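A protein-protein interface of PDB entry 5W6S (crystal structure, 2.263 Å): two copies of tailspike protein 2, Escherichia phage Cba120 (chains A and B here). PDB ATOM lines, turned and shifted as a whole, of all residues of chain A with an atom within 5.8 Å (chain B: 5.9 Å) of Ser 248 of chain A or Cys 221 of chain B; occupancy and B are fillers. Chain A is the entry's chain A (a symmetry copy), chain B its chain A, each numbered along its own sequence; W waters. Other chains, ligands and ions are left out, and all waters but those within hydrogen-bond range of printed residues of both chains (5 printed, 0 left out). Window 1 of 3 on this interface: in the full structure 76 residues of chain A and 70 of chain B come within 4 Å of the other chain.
The side-chain amide nitrogen of Asn 270 of chain A sits close to the side-chain hydroxyl of Thr 245 of chain B.
Water W1 lies within hydrogen-bond range of the side-chain carboxylate (OD2) of Asp 247 of chain A (2.5 Å), the side-chain carboxylate (OD2) of Asp 247 of chain B (3.2 Å) and the side-chain amino group (NZ) of Lys 224 of chain A (3.4 Å). Water W3 bridges the backbone carbonyl oxygen of Ser 248 of chain A (2.7 Å) and the side-chain sulfur of Cys 221 of chain B (3.7 Å). Water W5 bridges the side-chain carboxylate (OD1) of Asp 247 of chain B and the side-chain carboxylate (OD1) of Asp 247 of chain A. Water W2 bridges the side-chain amide nitrogen of Asn 270 of chain A (3.0 Å) and the backbone carbonyl oxygen of Thr 246 of chain B (3.2 Å). Water W4 bridges the side-chain hydroxyl of Ser 248 of chain A and the side-chain sulfur of Cys 221 of chain B.
Among the printed residues, pairs that only touch across the chains: Leu 146 of chain A with Val 172 of chain B, Lys 224 of chain A with Val 172 of chain B, Lys 224 of chain A with Ser 223 of chain B, Ser 248 of chain A with Cys 221 of chain B, Ser 248 of chain A with Thr 245 of chain B and Leu 250 of chain A with Asp 219 of chain B.
Of the 13 printed residues of chain B, 5 touch a printed residue of chain A. Of the 13 printed residues of chain A, 5 touch a printed residue of chain B.
Positions printed for both chains: 222, 223, 246 and 247. Of the 7 pairs that touch across the chains among the printed residues, none has its exchanged pair printed and touching as well.
The backbone NH (N) of Asp 219 of chain B sits at hydrogen-bond distance from the backbone carbonyl oxygen (O) of Ser 243 of chain B (3.3 Å). O of Thr 245 of chain B is in hydrogen-bond range of N of Ile 222 of chain B, at 2.8 Å. The side-chain carboxylate (OD2) of Asp 247 of chain B lies within hydrogen-bond range of the side-chain hydroxyl (OG) of Ser 223 of chain B (3.5 Å). The backbone carbonyl oxygen (O) of Asp 247 of chain A sits at hydrogen-bond distance from the backbone NH (N) of Lys 224 of chain A (2.8 Å). O of Thr 269 of chain A sits at hydrogen-bond distance from N of Ser 248 of chain A. OG of Ser 248 of chain A is in hydrogen-bond range of ND2 of Asn 270 of chain A.
Ser 248 of chain A touches just these residues of chain B: Cys 221 (3.9 Å) and Thr 245 (3.9 Å). Printed residues of chain B within 4 Å of Asn 270 of chain A: Thr 245 (3.1 Å). Of the printed residues of chain A, Val 172 of chain B touches Leu 146 and Lys 224. Leu 220 of chain B touches none of the printed residues of chain A. Of the printed residues of chain A, Cys 221 of chain B touches Ser 248. Of the printed residues of chain A, Ser 223 of chain B touches Lys 224. Of the printed residues of chain A, Thr 245 of chain B touches Ser 248 (3.9 Å) and Asn 270 (3.1 Å). The nearest residue of chain B that does not touch Ser 248 of chain A is Asp 247 of chain B (5.1 Å). The nearest printed residue of chain A that does not touch Cys 221 of chain B is Lys 224 of chain A (4.01 Å).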
ATOM      1  N   LEU A 146      29.845   5.545   1.980  1.00  0.00           N
ATOM      2  CA  LEU A 146      30.788   4.848   1.125  1.00  0.00           C
ATOM      3  C   LEU A 146      32.206   5.380   1.271  1.00  0.00           C
ATOM      4  O   LEU A 146      33.134   4.801   0.693  1.00  0.00           O
ATOM      5  CB  LEU A 146      30.328   4.948  -0.330  1.00  0.00           C
ATOM      6  CG  LEU A 146      29.236   3.947  -0.738  1.00  0.00           C
ATOM      7  CD1 LEU A 146      27.927   4.188   0.009  1.00  0.00           C
ATOM      8  CD2 LEU A 146      29.015   3.979  -2.245  1.00  0.00           C
ATOM      9  N   ILE A 222      27.090  -8.191   0.182  1.00  0.00           N
ATOM     10  CA  ILE A 222      27.976  -7.038   0.116  1.00  0.00           C
ATOM     11  C   ILE A 222      27.161  -5.918  -0.506  1.00  0.00           C
ATOM     12  O   ILE A 222      26.834  -5.961  -1.700  1.00  0.00           O
ATOM     13  CB  ILE A 222      29.244  -7.331  -0.688  1.00  0.00           C
ATOM     14  CG1 ILE A 222      29.968  -8.542  -0.086  1.00  0.00           C
ATOM     15  CG2 ILE A 222      30.149  -6.104  -0.695  1.00  0.00           C
ATOM     16  CD1 ILE A 222      31.153  -9.032  -0.928  1.00  0.00           C
ATOM     17  N   SER A 223      26.823  -4.922   0.307  1.00  0.00           N
ATOM     18  CA  SER A 223      25.762  -3.975  -0.005  1.00  0.00           C
ATOM     19  C   SER A 223      26.255  -2.555   0.236  1.00  0.00           C
ATOM     20  O   SER A 223      26.716  -2.233   1.337  1.00  0.00           O
ATOM     21  CB  SER A 223      24.523  -4.275   0.845  1.00  0.00           C
ATOM     22  OG  SER A 223      23.593  -3.219   0.791  1.00  0.00           O
ATOM     23  N   LYS A 224      26.145  -1.706  -0.788  1.00  0.00           N
ATOM     24  CA  LYS A 224      26.539  -0.299  -0.683  1.00  0.00           C
ATOM     25  C   LYS A 224      27.975  -0.179  -0.191  1.00  0.00           C
ATOM     26  O   LYS A 224      28.301   0.668   0.641  1.00  0.00           O
ATOM     27  CB  LYS A 224      25.596   0.489   0.232  1.00  0.00           C
ATOM     28  CG  LYS A 224      24.137   0.504  -0.196  1.00  0.00           C
ATOM     29  CD  LYS A 224      23.317   1.353   0.773  1.00  0.00           C
ATOM     30  CE  LYS A 224      21.841   0.943   0.800  1.00  0.00           C
ATOM     31  NZ  LYS A 224      21.613  -0.281   1.630  1.00  0.00           N
ATOM     32  N   VAL A 225      28.830  -1.044  -0.689  1.00  0.00           N
ATOM     33  CA  VAL A 225      30.233  -1.049  -0.313  1.00  0.00           C
ATOM     34  C   VAL A 225      31.040  -0.439  -1.450  1.00  0.00           C
ATOM     35  O   VAL A 225      30.785  -0.706  -2.631  1.00  0.00           O
ATOM     36  CB  VAL A 225      30.705  -2.473   0.039  1.00  0.00           C
ATOM     37  CG1 VAL A 225      32.234  -2.547   0.074  1.00  0.00           C
ATOM     38  CG2 VAL A 225      30.111  -2.881   1.392  1.00  0.00           C
ATOM     39  N   THR A 246      26.218  -9.233  -4.324  1.00  0.00           N
ATOM     40  CA  THR A 246      26.595  -7.828  -4.266  1.00  0.00           C
ATOM     41  C   THR A 246      25.389  -6.990  -4.654  1.00  0.00           C
ATOM     42  O   THR A 246      24.581  -7.384  -5.504  1.00  0.00           O
ATOM     43  CB  THR A 246      27.803  -7.487  -5.155  1.00  0.00           C
ATOM     44  OG1 THR A 246      27.413  -7.493  -6.532  1.00  0.00           O
ATOM     45  CG2 THR A 246      28.946  -8.490  -4.928  1.00  0.00           C
ATOM     46  N   ASP A 247      25.264  -5.844  -4.000  1.00  0.00           N
ATOM     47  CA  ASP A 247      24.127  -4.963  -4.199  1.00  0.00           C
ATOM     48  C   ASP A 247      24.631  -3.539  -4.045  1.00  0.00           C
ATOM     49  O   ASP A 247      25.109  -3.166  -2.968  1.00  0.00           O
ATOM     50  CB  ASP A 247      23.015  -5.272  -3.194  1.00  0.00           C
ATOM     51  CG  ASP A 247      21.946  -4.206  -3.167  1.00  0.00           C
ATOM     52  OD1 ASP A 247      21.387  -3.885  -4.241  1.00  0.00           O
ATOM     53  OD2 ASP A 247      21.674  -3.678  -2.069  1.00  0.00           O
ATOM     54  N   SER A 248      24.544  -2.756  -5.118  1.00  0.00           N
ATOM     55  CA  SER A 248      25.070  -1.395  -5.114  1.00  0.00           C
ATOM     56  C   SER A 248      26.553  -1.377  -4.758  1.00  0.00           C
ATOM     57  O   SER A 248      27.023  -0.509  -4.023  1.00  0.00           O
ATOM     58  CB  SER A 248      24.277  -0.498  -4.165  1.00  0.00           C
ATOM     59  OG  SER A 248      23.027  -0.166  -4.732  1.00  0.00           O
ATOM     60  N   LEU A 249      27.294  -2.353  -5.272  1.00  0.00           N
ATOM     61  CA  LEU A 249      28.743  -2.321  -5.158  1.00  0.00           C
ATOM     62  C   LEU A 249      29.298  -1.242  -6.074  1.00  0.00           C
ATOM     63  O   LEU A 249      28.865  -1.101  -7.222  1.00  0.00           O
ATOM     64  CB  LEU A 249      29.334  -3.681  -5.533  1.00  0.00           C
ATOM     65  CG  LEU A 249      30.854  -3.840  -5.446  1.00  0.00           C
ATOM     66  CD1 LEU A 249      31.332  -3.780  -3.992  1.00  0.00           C
ATOM     67  CD2 LEU A 249      31.317  -5.131  -6.130  1.00  0.00           C
ATOM     68  N   LEU A 250      30.253  -0.468  -5.562  1.00  0.00           N
ATOM     69  CA  LEU A 250      30.915   0.577  -6.334  1.00  0.00           C
ATOM     70  C   LEU A 250      32.416   0.346  -6.258  1.00  0.00           C
ATOM     71  O   LEU A 250      32.997   0.361  -5.167  1.00  0.00           O
ATOM     72  CB  LEU A 250      30.552   1.977  -5.817  1.00  0.00           C
ATOM     73  CG  LEU A 250      31.280   3.152  -6.493  1.00  0.00           C
ATOM     74  CD1 LEU A 250      30.907   3.277  -7.974  1.00  0.00           C
ATOM     75  CD2 LEU A 250      31.036   4.477  -5.759  1.00  0.00           C
ATOM     76  N   THR A 269      23.264  -7.131  -8.175  1.00  0.00           N
ATOM     77  CA  THR A 269      22.413  -6.065  -8.681  1.00  0.00           C
ATOM     78  C   THR A 269      23.112  -4.722  -8.523  1.00  0.00           C
ATOM     79  O   THR A 269      23.807  -4.479  -7.530  1.00  0.00           O
ATOM     80  CB  THR A 269      21.038  -6.045  -7.979  1.00  0.00           C
ATOM     81  OG1 THR A 269      21.218  -5.886  -6.569  1.00  0.00           O
ATOM     82  CG2 THR A 269      20.289  -7.352  -8.236  1.00  0.00           C
ATOM     83  N   ASN A 270      22.928  -3.866  -9.524  1.00  0.00           N
ATOM     84  CA  ASN A 270      23.433  -2.493  -9.542  1.00  0.00           C
ATOM     85  C   ASN A 270      24.900  -2.417  -9.125  1.00  0.00           C
ATOM     86  O   ASN A 270      25.262  -1.808  -8.114  1.00  0.00           O
ATOM     87  CB  ASN A 270      22.587  -1.569  -8.661  1.00  0.00           C
ATOM     88  CG  ASN A 270      23.036  -0.111  -8.761  1.00  0.00           C
ATOM     89  OD1 ASN A 270      23.683   0.284  -9.734  1.00  0.00           O
ATOM     90  ND2 ASN A 270      22.709   0.683  -7.754  1.00  0.00           N
ATOM     91  N   ILE A 271      25.751  -3.018  -9.944  1.00  0.00           N
ATOM     92  CA  ILE A 271      27.195  -2.934  -9.771  1.00  0.00           C
ATOM     93  C   ILE A 271      27.723  -1.843 -10.693  1.00  0.00           C
ATOM     94  O   ILE A 271      27.248  -1.690 -11.827  1.00  0.00           O
ATOM     95  CB  ILE A 271      27.870  -4.291 -10.059  1.00  0.00           C
ATOM     96  CG1 ILE A 271      29.390  -4.197  -9.874  1.00  0.00           C
ATOM     97  CG2 ILE A 271      27.526  -4.801 -11.474  1.00  0.00           C
ATOM     98  CD1 ILE A 271      30.105  -5.553 -10.016  1.00  0.00           C
ATOM     99  N   ILE B 171      27.438   9.357  -0.067  1.00  0.00           N
ATOM    100  CA  ILE B 171      26.626   9.249   1.124  1.00  0.00           C
ATOM    101  C   ILE B 171      25.548   8.192   0.905  1.00  0.00           C
ATOM    102  O   ILE B 171      25.324   7.716  -0.206  1.00  0.00           O
ATOM    103  CB  ILE B 171      25.989  10.600   1.517  1.00  0.00           C
ATOM    104  CG1 ILE B 171      25.050  11.071   0.403  1.00  0.00           C
ATOM    105  CG2 ILE B 171      27.074  11.633   1.832  1.00  0.00           C
ATOM    106  CD1 ILE B 171      24.130  12.187   0.814  1.00  0.00           C
ATOM    107  N   VAL B 172      24.858   7.838   1.983  1.00  0.00           N
ATOM    108  CA  VAL B 172      23.696   6.963   1.933  1.00  0.00           C
ATOM    109  C   VAL B 172      22.515   7.691   2.556  1.00  0.00           C
ATOM    110  O   VAL B 172      22.646   8.335   3.605  1.00  0.00           O
ATOM    111  CB  VAL B 172      23.956   5.628   2.660  1.00  0.00           C
ATOM    112  CG1 VAL B 172      22.686   4.785   2.700  1.00  0.00           C
ATOM    113  CG2 VAL B 172      25.087   4.872   1.977  1.00  0.00           C
ATOM    114  N   LEU B 173      21.373   7.607   1.892  1.00  0.00           N
ATOM    115  CA  LEU B 173      20.082   7.987   2.453  1.00  0.00           C
ATOM    116  C   LEU B 173      19.283   6.694   2.541  1.00  0.00           C
ATOM    117  O   LEU B 173      18.975   6.085   1.509  1.00  0.00           O
ATOM    118  CB  LEU B 173      19.377   9.032   1.589  1.00  0.00           C
ATOM    119  CG  LEU B 173      20.152  10.324   1.274  1.00  0.00           C
ATOM    120  CD1 LEU B 173      19.308  11.294   0.453  1.00  0.00           C
ATOM    121  CD2 LEU B 173      20.623  10.999   2.550  1.00  0.00           C
ATOM    122  N   ASP B 174      18.976   6.255   3.763  1.00  0.00           N
ATOM    123  CA  ASP B 174      18.415   4.921   3.949  1.00  0.00           C
ATOM    124  C   ASP B 174      17.271   4.929   4.951  1.00  0.00           C
ATOM    125  O   ASP B 174      17.436   5.380   6.089  1.00  0.00           O
ATOM    126  CB  ASP B 174      19.494   3.931   4.409  1.00  0.00           C
ATOM    127  CG  ASP B 174      18.975   2.507   4.498  1.00  0.00           C
ATOM    128  OD1 ASP B 174      18.664   1.906   3.450  1.00  0.00           O
ATOM    129  OD2 ASP B 174      18.864   1.982   5.621  1.00  0.00           O
ATOM    130  N   ASP B 219      27.638   9.455  -6.872  1.00  0.00           N
ATOM    131  CA  ASP B 219      28.032   8.135  -6.374  1.00  0.00           C
ATOM    132  C   ASP B 219      27.415   7.847  -5.004  1.00  0.00           C
ATOM    133  O   ASP B 219      28.092   7.454  -4.050  1.00  0.00           O
ATOM    134  CB  ASP B 219      29.558   8.003  -6.333  1.00  0.00           C
ATOM    135  CG  ASP B 219      30.206   8.140  -7.719  1.00  0.00           C
ATOM    136  OD1 ASP B 219      29.518   8.548  -8.686  1.00  0.00           O
ATOM    137  OD2 ASP B 219      31.413   7.840  -7.834  1.00  0.00           O
ATOM    138  N   LEU B 220      26.107   8.040  -4.912  1.00  0.00           N
ATOM    139  CA  LEU B 220      25.409   7.914  -3.645  1.00  0.00           C
ATOM    140  C   LEU B 220      24.166   7.056  -3.839  1.00  0.00           C
ATOM    141  O   LEU B 220      23.694   6.860  -4.961  1.00  0.00           O
ATOM    142  CB  LEU B 220      25.047   9.299  -3.078  1.00  0.00           C
ATOM    143  CG  LEU B 220      24.151  10.215  -3.914  1.00  0.00           C
ATOM    144  CD1 LEU B 220      22.678   9.829  -3.761  1.00  0.00           C
ATOM    145  CD2 LEU B 220      24.377  11.680  -3.543  1.00  0.00           C
ATOM    146  N   CYS B 221      23.645   6.539  -2.729  1.00  0.00           N
ATOM    147  CA  CYS B 221      22.519   5.612  -2.738  1.00  0.00           C
ATOM    148  C   CYS B 221      21.343   6.225  -2.000  1.00  0.00           C
ATOM    149  O   CYS B 221      21.474   6.631  -0.839  1.00  0.00           O
ATOM    150  CB  CYS B 221      22.893   4.279  -2.092  1.00  0.00           C
ATOM    151  SG  CYS B 221      23.980   3.273  -3.096  1.00  0.00           S
ATOM    152  N   ILE B 222      20.203   6.300  -2.677  1.00  0.00           N
ATOM    153  CA  ILE B 222      18.931   6.637  -2.053  1.00  0.00           C
ATOM    154  C   ILE B 222      18.150   5.338  -1.965  1.00  0.00           C
ATOM    155  O   ILE B 222      17.709   4.793  -2.987  1.00  0.00           O
ATOM    156  CB  ILE B 222      18.169   7.706  -2.837  1.00  0.00           C
ATOM    157  CG1 ILE B 222      19.047   8.953  -2.995  1.00  0.00           C
ATOM    158  CG2 ILE B 222      16.866   8.044  -2.122  1.00  0.00           C
ATOM    159  CD1 ILE B 222      18.446  10.015  -3.926  1.00  0.00           C
ATOM    160  N   SER B 223      17.990   4.834  -0.745  1.00  0.00           N
ATOM    161  CA  SER B 223      17.605   3.450  -0.507  1.00  0.00           C
ATOM    162  C   SER B 223      16.471   3.401   0.507  1.00  0.00           C
ATOM    163  O   SER B 223      16.600   3.936   1.614  1.00  0.00           O
ATOM    164  CB  SER B 223      18.813   2.645  -0.016  1.00  0.00           C
ATOM    165  OG  SER B 223      18.423   1.395   0.500  1.00  0.00           O
ATOM    166  N   SER B 243      25.552   8.747 -11.401  1.00  0.00           N
ATOM    167  CA  SER B 243      25.521   7.645 -10.433  1.00  0.00           C
ATOM    168  C   SER B 243      24.733   7.996  -9.172  1.00  0.00           C
ATOM    169  O   SER B 243      25.113   7.619  -8.059  1.00  0.00           O
ATOM    170  CB  SER B 243      26.935   7.188 -10.061  1.00  0.00           C
ATOM    171  OG  SER B 243      27.719   6.917 -11.214  1.00  0.00           O
ATOM    172  N   THR B 245      22.125   6.542  -7.441  1.00  0.00           N
ATOM    173  CA  THR B 245      21.401   5.284  -7.359  1.00  0.00           C
ATOM    174  C   THR B 245      20.133   5.455  -6.526  1.00  0.00           C
ATOM    175  O   THR B 245      20.153   6.075  -5.456  1.00  0.00           O
ATOM    176  CB  THR B 245      22.289   4.212  -6.730  1.00  0.00           C
ATOM    177  OG1 THR B 245      23.251   3.760  -7.689  1.00  0.00           O
ATOM    178  CG2 THR B 245      21.447   3.022  -6.208  1.00  0.00           C
ATOM    179  N   THR B 246      19.022   4.911  -7.017  1.00  0.00           N
ATOM    180  CA  THR B 246      17.856   4.723  -6.165  1.00  0.00           C
ATOM    181  C   THR B 246      17.574   3.234  -6.057  1.00  0.00           C
ATOM    182  O   THR B 246      17.781   2.471  -7.008  1.00  0.00           O
ATOM    183  CB  THR B 246      16.611   5.476  -6.666  1.00  0.00           C
ATOM    184  OG1 THR B 246      16.076   4.822  -7.821  1.00  0.00           O
ATOM    185  CG2 THR B 246      16.958   6.936  -7.003  1.00  0.00           C
ATOM    186  N   ASP B 247      17.129   2.828  -4.876  1.00  0.00           N
ATOM    187  CA  ASP B 247      16.883   1.427  -4.585  1.00  0.00           C
ATOM    188  C   ASP B 247      15.697   1.367  -3.640  1.00  0.00           C
ATOM    189  O   ASP B 247      15.769   1.892  -2.523  1.00  0.00           O
ATOM    190  CB  ASP B 247      18.121   0.774  -3.967  1.00  0.00           C
ATOM    191  CG  ASP B 247      17.828  -0.587  -3.382  1.00  0.00           C
ATOM    192  OD1 ASP B 247      17.285  -1.451  -4.109  1.00  0.00           O
ATOM    193  OD2 ASP B 247      18.129  -0.788  -2.188  1.00  0.00           O
HETATM  194  O   HOH W   1      21.197  -1.286  -1.585  1.00  0.00           O
HETATM  195  O   HOH W   2      19.801   0.048  -7.231  1.00  0.00           O
HETATM  196  O   HOH W   3      26.915   2.002  -5.043  1.00  0.00           O
HETATM  197  O   HOH W   4      21.302   1.126  -2.481  1.00  0.00           O
HETATM  198  O   HOH W   5      18.839  -3.571  -2.970  1.00  0.00           O
